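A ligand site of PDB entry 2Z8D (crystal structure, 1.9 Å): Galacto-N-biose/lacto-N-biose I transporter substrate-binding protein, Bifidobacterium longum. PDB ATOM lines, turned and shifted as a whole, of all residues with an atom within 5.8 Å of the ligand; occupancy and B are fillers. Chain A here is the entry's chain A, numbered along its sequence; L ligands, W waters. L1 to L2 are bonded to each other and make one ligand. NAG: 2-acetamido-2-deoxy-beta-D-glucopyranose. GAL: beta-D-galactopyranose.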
ATOM      1  N   ARG A  23     -12.952 -12.643  27.713  1.00  0.00           N
ATOM      2  CA  ARG A  23     -12.718 -11.806  26.528  1.00  0.00           C
ATOM      3  C   ARG A  23     -13.696 -12.116  25.391  1.00  0.00           C
ATOM      4  O   ARG A  23     -13.370 -12.162  24.202  1.00  0.00           O
ATOM      5  CB  ARG A  23     -11.223 -11.862  26.128  1.00  0.00           C
ATOM      6  CG  ARG A  23     -10.649 -13.334  25.803  1.00  0.00           C
ATOM      7  CD  ARG A  23      -9.168 -13.199  25.474  1.00  0.00           C
ATOM      8  NE  ARG A  23      -8.397 -14.454  25.402  1.00  0.00           N
ATOM      9  CZ  ARG A  23      -8.351 -15.254  24.338  1.00  0.00           C
ATOM     10  NH1 ARG A  23      -9.037 -14.990  23.236  1.00  0.00           N
ATOM     11  NH2 ARG A  23      -7.596 -16.353  24.371  1.00  0.00           N
ATOM     12  N   LEU A  24     -14.949 -12.362  25.780  1.00  0.00           N
ATOM     13  CA  LEU A  24     -16.032 -12.528  24.880  1.00  0.00           C
ATOM     14  C   LEU A  24     -16.412 -11.157  24.345  1.00  0.00           C
ATOM     15  O   LEU A  24     -16.245 -10.150  25.067  1.00  0.00           O
ATOM     16  CB  LEU A  24     -17.194 -13.207  25.625  1.00  0.00           C
ATOM     17  CG  LEU A  24     -16.889 -14.680  26.078  1.00  0.00           C
ATOM     18  CD1 LEU A  24     -18.135 -15.207  26.796  1.00  0.00           C
ATOM     19  CD2 LEU A  24     -16.556 -15.521  24.849  1.00  0.00           C
ATOM     20  N   PRO A  25     -16.904 -11.113  23.097  1.00  0.00           N
ATOM     21  CA  PRO A  25     -17.139  -9.837  22.402  1.00  0.00           C
ATOM     22  C   PRO A  25     -18.132  -8.891  23.017  1.00  0.00           C
ATOM     23  O   PRO A  25     -17.874  -7.668  22.959  1.00  0.00           O
ATOM     24  CB  PRO A  25     -17.536 -10.247  20.992  1.00  0.00           C
ATOM     25  CG  PRO A  25     -17.965 -11.676  21.107  1.00  0.00           C
ATOM     26  CD  PRO A  25     -17.127 -12.268  22.197  1.00  0.00           C
ATOM     27  N   LYS A  57      -5.891  -6.409  23.555  1.00  0.00           N
ATOM     28  CA  LYS A  57      -5.775  -7.361  22.447  1.00  0.00           C
ATOM     29  C   LYS A  57      -5.852  -8.775  23.056  1.00  0.00           C
ATOM     30  O   LYS A  57      -5.268  -9.027  24.107  1.00  0.00           O
ATOM     31  CB  LYS A  57      -4.434  -7.104  21.752  1.00  0.00           C
ATOM     32  CG  LYS A  57      -4.074  -7.945  20.602  1.00  0.00           C
ATOM     33  CD  LYS A  57      -2.671  -7.615  20.082  1.00  0.00           C
ATOM     34  CE  LYS A  57      -2.389  -8.363  18.777  1.00  0.00           C
ATOM     35  NZ  LYS A  57      -2.372  -9.877  18.850  1.00  0.00           N
ATOM     36  N   ALA A  58      -6.610  -9.668  22.419  1.00  0.00           N
ATOM     37  CA  ALA A  58      -6.874 -11.024  22.962  1.00  0.00           C
ATOM     38  C   ALA A  58      -5.616 -11.729  23.487  1.00  0.00           C
ATOM     39  O   ALA A  58      -5.600 -12.216  24.622  1.00  0.00           O
ATOM     40  CB  ALA A  58      -7.648 -11.887  21.915  1.00  0.00           C
ATOM     41  N   SER A  59      -4.560 -11.758  22.676  1.00  0.00           N
ATOM     42  CA  SER A  59      -3.282 -12.414  23.004  1.00  0.00           C
ATOM     43  C   SER A  59      -2.600 -11.842  24.243  1.00  0.00           C
ATOM     44  O   SER A  59      -1.715 -12.466  24.788  1.00  0.00           O
ATOM     45  CB  SER A  59      -2.300 -12.337  21.801  1.00  0.00           C
ATOM     46  OG  SER A  59      -2.227 -10.987  21.326  1.00  0.00           O
ATOM     47  N   GLN A  79     -10.918 -16.757  31.195  1.00  0.00           N
ATOM     48  CA  GLN A  79     -10.798 -17.369  29.871  1.00  0.00           C
ATOM     49  C   GLN A  79      -9.346 -17.634  29.520  1.00  0.00           C
ATOM     50  O   GLN A  79      -8.495 -16.732  29.599  1.00  0.00           O
ATOM     51  CB  GLN A  79     -11.460 -16.481  28.813  1.00  0.00           C
ATOM     52  CG  GLN A  79     -11.566 -17.172  27.405  1.00  0.00           C
ATOM     53  CD  GLN A  79     -12.273 -16.288  26.382  1.00  0.00           C
ATOM     54  OE1 GLN A  79     -12.965 -15.347  26.751  1.00  0.00           O
ATOM     55  NE2 GLN A  79     -12.072 -16.584  25.082  1.00  0.00           N
ATOM     56  N   GLU A  84      -3.364 -21.750  24.944  1.00  0.00           N
ATOM     57  CA  GLU A  84      -2.685 -21.052  26.026  1.00  0.00           C
ATOM     58  C   GLU A  84      -2.568 -21.839  27.324  1.00  0.00           C
ATOM     59  O   GLU A  84      -1.762 -21.500  28.196  1.00  0.00           O
ATOM     60  CB  GLU A  84      -3.416 -19.739  26.353  1.00  0.00           C
ATOM     61  CG  GLU A  84      -3.488 -18.787  25.154  1.00  0.00           C
ATOM     62  CD  GLU A  84      -4.345 -17.527  25.407  1.00  0.00           C
ATOM     63  OE1 GLU A  84      -5.398 -17.604  26.088  1.00  0.00           O
ATOM     64  OE2 GLU A  84      -3.983 -16.463  24.858  1.00  0.00           O
ATOM     65  N   GLN A 127     -15.190 -24.286  27.065  1.00  0.00           N
ATOM     66  CA  GLN A 127     -16.297 -23.351  26.756  1.00  0.00           C
ATOM     67  C   GLN A 127     -16.755 -23.424  25.289  1.00  0.00           C
ATOM     68  O   GLN A 127     -17.948 -23.511  25.022  1.00  0.00           O
ATOM     69  CB  GLN A 127     -15.962 -21.922  27.202  1.00  0.00           C
ATOM     70  CG  GLN A 127     -17.103 -20.933  26.984  1.00  0.00           C
ATOM     71  CD  GLN A 127     -16.778 -19.562  27.547  1.00  0.00           C
ATOM     72  OE1 GLN A 127     -16.030 -18.787  26.924  1.00  0.00           O
ATOM     73  NE2 GLN A 127     -17.279 -19.292  28.769  1.00  0.00           N
ATOM     74  N   ASP A 128     -15.817 -23.414  24.341  1.00  0.00           N
ATOM     75  CA  ASP A 128     -16.177 -23.445  22.900  1.00  0.00           C
ATOM     76  C   ASP A 128     -15.121 -24.085  22.029  1.00  0.00           C
ATOM     77  O   ASP A 128     -14.014 -24.388  22.491  1.00  0.00           O
ATOM     78  CB  ASP A 128     -16.419 -21.997  22.388  1.00  0.00           C
ATOM     79  CG  ASP A 128     -15.126 -21.136  22.428  1.00  0.00           C
ATOM     80  OD1 ASP A 128     -14.455 -21.097  23.482  1.00  0.00           O
ATOM     81  OD2 ASP A 128     -14.799 -20.490  21.408  1.00  0.00           O
ATOM     82  N   ASP A 176      -1.851 -10.489  10.873  1.00  0.00           N
ATOM     83  CA  ASP A 176      -2.073 -10.372  12.333  1.00  0.00           C
ATOM     84  C   ASP A 176      -2.730 -11.640  12.979  1.00  0.00           C
ATOM     85  O   ASP A 176      -2.841 -11.718  14.195  1.00  0.00           O
ATOM     86  CB  ASP A 176      -2.902  -9.157  12.694  1.00  0.00           C
ATOM     87  CG  ASP A 176      -4.290  -9.138  12.029  1.00  0.00           C
ATOM     88  OD1 ASP A 176      -4.504  -9.868  11.044  1.00  0.00           O
ATOM     89  OD2 ASP A 176      -5.147  -8.360  12.466  1.00  0.00           O
ATOM     90  N   GLU A 177      -3.129 -12.589  12.128  1.00  0.00           N
ATOM     91  CA  GLU A 177      -3.757 -13.831  12.587  1.00  0.00           C
ATOM     92  C   GLU A 177      -3.013 -15.095  12.140  1.00  0.00           C
ATOM     93  O   GLU A 177      -3.556 -16.167  12.308  1.00  0.00           O
ATOM     94  CB  GLU A 177      -5.242 -13.876  12.129  1.00  0.00           C
ATOM     95  CG  GLU A 177      -6.212 -13.026  13.013  1.00  0.00           C
ATOM     96  CD  GLU A 177      -6.318 -13.553  14.444  1.00  0.00           C
ATOM     97  OE1 GLU A 177      -6.300 -14.814  14.613  1.00  0.00           O
ATOM     98  OE2 GLU A 177      -6.368 -12.737  15.405  1.00  0.00           O
ATOM     99  N   ASN A 180      -2.628 -17.946  14.674  1.00  0.00           N
ATOM    100  CA  ASN A 180      -3.839 -18.700  15.086  1.00  0.00           C
ATOM    101  C   ASN A 180      -4.469 -19.404  13.911  1.00  0.00           C
ATOM    102  O   ASN A 180      -4.762 -20.592  13.968  1.00  0.00           O
ATOM    103  CB  ASN A 180      -4.818 -17.761  15.760  1.00  0.00           C
ATOM    104  CG  ASN A 180      -4.191 -17.021  16.925  1.00  0.00           C
ATOM    105  OD1 ASN A 180      -3.414 -17.574  17.665  1.00  0.00           O
ATOM    106  ND2 ASN A 180      -4.561 -15.747  17.086  1.00  0.00           N
ATOM    107  N   TRP A 231      -8.022  -7.375  12.096  1.00  0.00           N
ATOM    108  CA  TRP A 231      -8.626  -6.507  13.101  1.00  0.00           C
ATOM    109  C   TRP A 231      -8.507  -5.037  12.756  1.00  0.00           C
ATOM    110  O   TRP A 231      -8.872  -4.188  13.562  1.00  0.00           O
ATOM    111  CB  TRP A 231      -8.084  -6.833  14.512  1.00  0.00           C
ATOM    112  CG  TRP A 231      -8.218  -8.296  14.744  1.00  0.00           C
ATOM    113  CD1 TRP A 231      -7.201  -9.182  14.856  1.00  0.00           C
ATOM    114  CD2 TRP A 231      -9.440  -9.055  14.756  1.00  0.00           C
ATOM    115  NE1 TRP A 231      -7.706 -10.461  14.984  1.00  0.00           N
ATOM    116  CE2 TRP A 231      -9.074 -10.411  14.920  1.00  0.00           C
ATOM    117  CE3 TRP A 231     -10.805  -8.719  14.644  1.00  0.00           C
ATOM    118  CZ2 TRP A 231     -10.024 -11.445  14.963  1.00  0.00           C
ATOM    119  CZ3 TRP A 231     -11.758  -9.732  14.716  1.00  0.00           C
ATOM    120  CH2 TRP A 231     -11.355 -11.098  14.877  1.00  0.00           C
ATOM    121  N   TRP A 252     -16.353 -19.073  15.131  1.00  0.00           N
ATOM    122  CA  TRP A 252     -16.792 -18.011  16.076  1.00  0.00           C
ATOM    123  C   TRP A 252     -16.805 -16.583  15.478  1.00  0.00           C
ATOM    124  O   TRP A 252     -17.248 -15.596  16.153  1.00  0.00           O
ATOM    125  CB  TRP A 252     -15.996 -18.041  17.409  1.00  0.00           C
ATOM    126  CG  TRP A 252     -14.461 -18.153  17.273  1.00  0.00           C
ATOM    127  CD1 TRP A 252     -13.701 -19.331  17.455  1.00  0.00           C
ATOM    128  CD2 TRP A 252     -13.538 -17.145  16.872  1.00  0.00           C
ATOM    129  NE1 TRP A 252     -12.363 -19.053  17.223  1.00  0.00           N
ATOM    130  CE2 TRP A 252     -12.234 -17.731  16.865  1.00  0.00           C
ATOM    131  CE3 TRP A 252     -13.664 -15.766  16.544  1.00  0.00           C
ATOM    132  CZ2 TRP A 252     -11.070 -17.006  16.491  1.00  0.00           C
ATOM    133  CZ3 TRP A 252     -12.495 -15.052  16.176  1.00  0.00           C
ATOM    134  CH2 TRP A 252     -11.236 -15.650  16.190  1.00  0.00           C
ATOM    135  N   LEU A 256     -19.177 -11.415  14.429  1.00  0.00           N
ATOM    136  CA  LEU A 256     -18.155 -10.371  14.214  1.00  0.00           C
ATOM    137  C   LEU A 256     -18.106  -9.914  12.747  1.00  0.00           C
ATOM    138  O   LEU A 256     -18.157  -8.697  12.435  1.00  0.00           O
ATOM    139  CB  LEU A 256     -16.786 -10.885  14.675  1.00  0.00           C
ATOM    140  CG  LEU A 256     -16.675 -11.665  16.009  1.00  0.00           C
ATOM    141  CD1 LEU A 256     -15.208 -11.962  16.329  1.00  0.00           C
ATOM    142  CD2 LEU A 256     -17.308 -10.817  17.158  1.00  0.00           C
ATOM    143  N   ASP A 287      -8.650 -22.953  15.265  1.00  0.00           N
ATOM    144  CA  ASP A 287      -8.236 -21.574  15.357  1.00  0.00           C
ATOM    145  C   ASP A 287      -8.970 -20.972  16.574  1.00  0.00           C
ATOM    146  O   ASP A 287     -10.196 -20.753  16.559  1.00  0.00           O
ATOM    147  CB  ASP A 287      -8.522 -20.878  14.019  1.00  0.00           C
ATOM    148  CG  ASP A 287      -8.314 -19.378  14.069  1.00  0.00           C
ATOM    149  OD1 ASP A 287      -7.942 -18.828  15.126  1.00  0.00           O
ATOM    150  OD2 ASP A 287      -8.557 -18.728  13.030  1.00  0.00           O
ATOM    151  N   GLY A 288      -8.230 -20.780  17.663  1.00  0.00           N
ATOM    152  CA  GLY A 288      -8.822 -20.375  18.898  1.00  0.00           C
ATOM    153  C   GLY A 288      -9.684 -21.504  19.484  1.00  0.00           C
ATOM    154  O   GLY A 288      -9.428 -22.697  19.230  1.00  0.00           O
ATOM    155  N   GLY A 289     -10.692 -21.126  20.263  1.00  0.00           N
ATOM    156  CA  GLY A 289     -11.457 -22.097  21.094  1.00  0.00           C
ATOM    157  C   GLY A 289     -10.858 -22.006  22.479  1.00  0.00           C
ATOM    158  O   GLY A 289      -9.621 -21.882  22.657  1.00  0.00           O
ATOM    159  N   SER A 290     -11.697 -22.014  23.496  1.00  0.00           N
ATOM    160  CA  SER A 290     -11.239 -21.584  24.817  1.00  0.00           C
ATOM    161  C   SER A 290     -11.873 -22.404  25.934  1.00  0.00           C
ATOM    162  O   SER A 290     -12.987 -22.895  25.796  1.00  0.00           O
ATOM    163  CB  SER A 290     -11.579 -20.093  25.043  1.00  0.00           C
ATOM    164  OG  SER A 290     -10.917 -19.236  24.080  1.00  0.00           O
ATOM    165  N   GLN A 321     -22.907 -15.038  21.381  1.00  0.00           N
ATOM    166  CA  GLN A 321     -21.562 -14.469  21.351  1.00  0.00           C
ATOM    167  C   GLN A 321     -20.695 -14.913  20.172  1.00  0.00           C
ATOM    168  O   GLN A 321     -19.514 -14.523  20.075  1.00  0.00           O
ATOM    169  CB  GLN A 321     -20.841 -14.708  22.678  1.00  0.00           C
ATOM    170  CG  GLN A 321     -21.498 -14.038  23.924  1.00  0.00           C
ATOM    171  CD  GLN A 321     -21.103 -12.570  24.145  1.00  0.00           C
ATOM    172  OE1 GLN A 321     -20.042 -12.109  23.683  1.00  0.00           O
ATOM    173  NE2 GLN A 321     -21.896 -11.876  24.962  1.00  0.00           N
ATOM    174  N   LEU A 323     -20.135 -18.158  19.820  1.00  0.00           N
ATOM    175  CA  LEU A 323     -19.480 -19.406  20.275  1.00  0.00           C
ATOM    176  C   LEU A 323     -20.103 -20.684  19.701  1.00  0.00           C
ATOM    177  O   LEU A 323     -21.352 -20.803  19.474  1.00  0.00           O
ATOM    178  CB  LEU A 323     -19.439 -19.492  21.802  1.00  0.00           C
ATOM    179  CG  LEU A 323     -18.766 -18.355  22.580  1.00  0.00           C
ATOM    180  CD1 LEU A 323     -18.609 -18.702  24.037  1.00  0.00           C
ATOM    181  CD2 LEU A 323     -17.430 -17.974  21.933  1.00  0.00           C
HETATM  182  C1  NAG L   1      -8.101 -13.333  17.980  1.00  0.00           C
HETATM  183  C2  NAG L   1      -8.500 -14.292  19.093  1.00  0.00           C
HETATM  184  C3  NAG L   1     -10.039 -14.346  19.224  1.00  0.00           C
HETATM  185  C4  NAG L   1     -10.641 -12.924  19.369  1.00  0.00           C
HETATM  186  C5  NAG L   1     -10.036 -12.012  18.277  1.00  0.00           C
HETATM  187  C6  NAG L   1     -10.509 -10.543  18.342  1.00  0.00           C
HETATM  188  C7  NAG L   1      -7.333 -16.333  19.809  1.00  0.00           C
HETATM  189  C8  NAG L   1      -6.796 -17.699  19.439  1.00  0.00           C
HETATM  190  N2  NAG L   1      -7.927 -15.636  18.838  1.00  0.00           N
HETATM  191  O1  NAG L   1      -6.718 -13.224  17.989  1.00  0.00           O
HETATM  192  O3  NAG L   1     -10.346 -15.131  20.360  1.00  0.00           O
HETATM  193  O4  NAG L   1     -12.010 -13.037  19.149  1.00  0.00           O
HETATM  194  O5  NAG L   1      -8.609 -12.065  18.366  1.00  0.00           O
HETATM  195  O6  NAG L   1     -10.207  -9.978  19.621  1.00  0.00           O
HETATM  196  O7  NAG L   1      -7.216 -15.894  20.956  1.00  0.00           O
HETATM  197  C1  GAL L   2     -11.515 -15.964  20.171  1.00  0.00           C
HETATM  198  C2  GAL L   2     -11.390 -17.236  21.031  1.00  0.00           C
HETATM  199  C3  GAL L   2     -12.719 -18.004  21.041  1.00  0.00           C
HETATM  200  C4  GAL L   2     -13.851 -17.104  21.467  1.00  0.00           C
HETATM  201  C5  GAL L   2     -13.904 -15.860  20.534  1.00  0.00           C
HETATM  202  C6  GAL L   2     -14.912 -14.857  21.018  1.00  0.00           C
HETATM  203  O2  GAL L   2     -10.413 -18.096  20.555  1.00  0.00           O
HETATM  204  O3  GAL L   2     -12.631 -19.189  21.818  1.00  0.00           O
HETATM  205  O4  GAL L   2     -13.673 -16.743  22.833  1.00  0.00           O
HETATM  206  O5  GAL L   2     -12.602 -15.205  20.564  1.00  0.00           O
HETATM  207  O6  GAL L   2     -15.172 -13.888  20.002  1.00  0.00           O
HETATM  208  O   HOH W   1     -17.197 -14.562  18.537  1.00  0.00           O
HETATM  209  O   HOH W   2      -8.688 -18.458  22.547  1.00  0.00           O
HETATM  210  O   HOH W   3      -4.726 -14.075  19.637  1.00  0.00           O
HETATM  211  O   HOH W   4     -14.173 -11.140  19.881  1.00  0.00           O
HETATM  212  O   HOH W   5      -7.830  -9.001  19.709  1.00  0.00           O
HETATM  213  O   HOH W   6     -14.552 -18.798  24.544  1.00  0.00           O
HETATM  214  O   HOH W   7      -4.751 -16.112  22.078  1.00  0.00           O
HETATM  215  O   HOH W   8     -11.453 -13.417  22.679  1.00  0.00           O
HETATM  216  O   HOH W   9     -11.323  -9.342  22.161  1.00  0.00           O
HETATM  217  O   HOH W  10      -4.791 -11.179  19.690  1.00  0.00           O
HETATM  218  O   HOH W  11      -6.335 -10.153  18.053  1.00  0.00           O
HETATM  219  O   HOH W  12      -7.931 -16.209  16.248  1.00  0.00           O
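O3 of GAL L2 is in hydrogen-bond range of OD2 of Asp 128, at 2.6 Å.
The side-chain carboxylate of Glu 177 sits at hydrogen-bond distance from an oxygen (O1) of NAG L1 (2.7 Å).
An oxygen (O4) of GAL L2 lies within hydrogen-bond range of the side-chain amide nitrogen of Gln 79, 2.8 Å away.
N of Ser 290 lies within hydrogen-bond range of O3 of GAL L2, 3.4 Å away.
The side-chain hydroxyl of Ser 290 sits at hydrogen-bond distance from an oxygen (O3) of GAL L2, at 2.8 Å.
The guanidinium group (NH1) of Arg 23 sits at hydrogen-bond distance from an oxygen (O7) of NAG L1 (3.1 Å).
O2 of GAL L2 is in hydrogen-bond range of N of Gly 289, at 3.1 Å.
ND2 of Asn 180 is in hydrogen-bond range of O1 of NAG L1 (3.4 Å).
The side-chain carboxylate (OD1) of Asp 128 is in hydrogen-bond range of the backbone NH (N) of Ser 290 (2.9 Å).
The side-chain carboxylate (OE2) of Glu 177 is in hydrogen-bond range of the indole nitrogen (NE1) of Trp 231.
The side-chain carboxylate (OE1) of Glu 177 is in hydrogen-bond range of the side-chain amide nitrogen (ND2) of Asn 180 (3.2 Å).
The side-chain amide nitrogen (NE2) of Gln 79 is in hydrogen-bond range of the side-chain hydroxyl (OG) of Ser 290, 3.1 Å away.
The side-chain amide oxygen of Gln 79 sits at hydrogen-bond distance from the backbone NH of Arg 23 (2.9 Å).
The backbone NH (N) of Gln 127 sits at hydrogen-bond distance from the backbone carbonyl oxygen (O) of Ser 290.
N of Trp 231 lies within hydrogen-bond range of OD2 of Asp 176, 3.1 Å away.
NE1 of Trp 252 lies within hydrogen-bond range of O of Asp 287 (2.8 Å).
CD2 of Leu 24 touches O4 of GAL L2, 3.7 Å away.
CD of Pro 25 touches O6 of GAL L2 (3.4 Å).
CB of Ala 58 touches O5 of NAG L1 (3.7 Å).
CZ2 of Trp 231 touches C5 of NAG L1 (3.4 Å).
Trp 252 touches the ligand.
CA of Gly 288 touches O2 of GAL L2, at 3.2 Å.
Leu 323 touches the ligand.
Of the 22 residues printed, 14 come within 4 Å of the ligand.
The nearest printed residue that does not touch the ligand is Leu 256 (4.1 Å).
Water W12 lies within hydrogen-bond range of N2 of NAG L1, OE1 of Glu 177 and OD1 of Asp 287.
Water W2 lies within hydrogen-bond range of an oxygen (O2) of GAL L2 (2.7 Å), the side-chain hydroxyl (OG) of Ser 290 (2.8 Å) and the guanidinium group (NH2) of Arg 23 (3.0 Å).
Water W7 lies within hydrogen-bond range of O7 of NAG L1 (2.7 Å) and OE2 of Glu 84 (2.9 Å).
Water W11 bridges an oxygen (O5) of NAG L1 (3.0 Å) and the indole nitrogen of Trp 231 (3.4 Å).
Water W8 bridges O of Arg 23 (2.8 Å) and O5 of GAL L2 (3.0 Å).
Water W10 lies within hydrogen-bond range of NZ of Lys 57 (2.9 Å), OG of Ser 59 (3.0 Å) and O1 of NAG L1 (3.3 Å).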
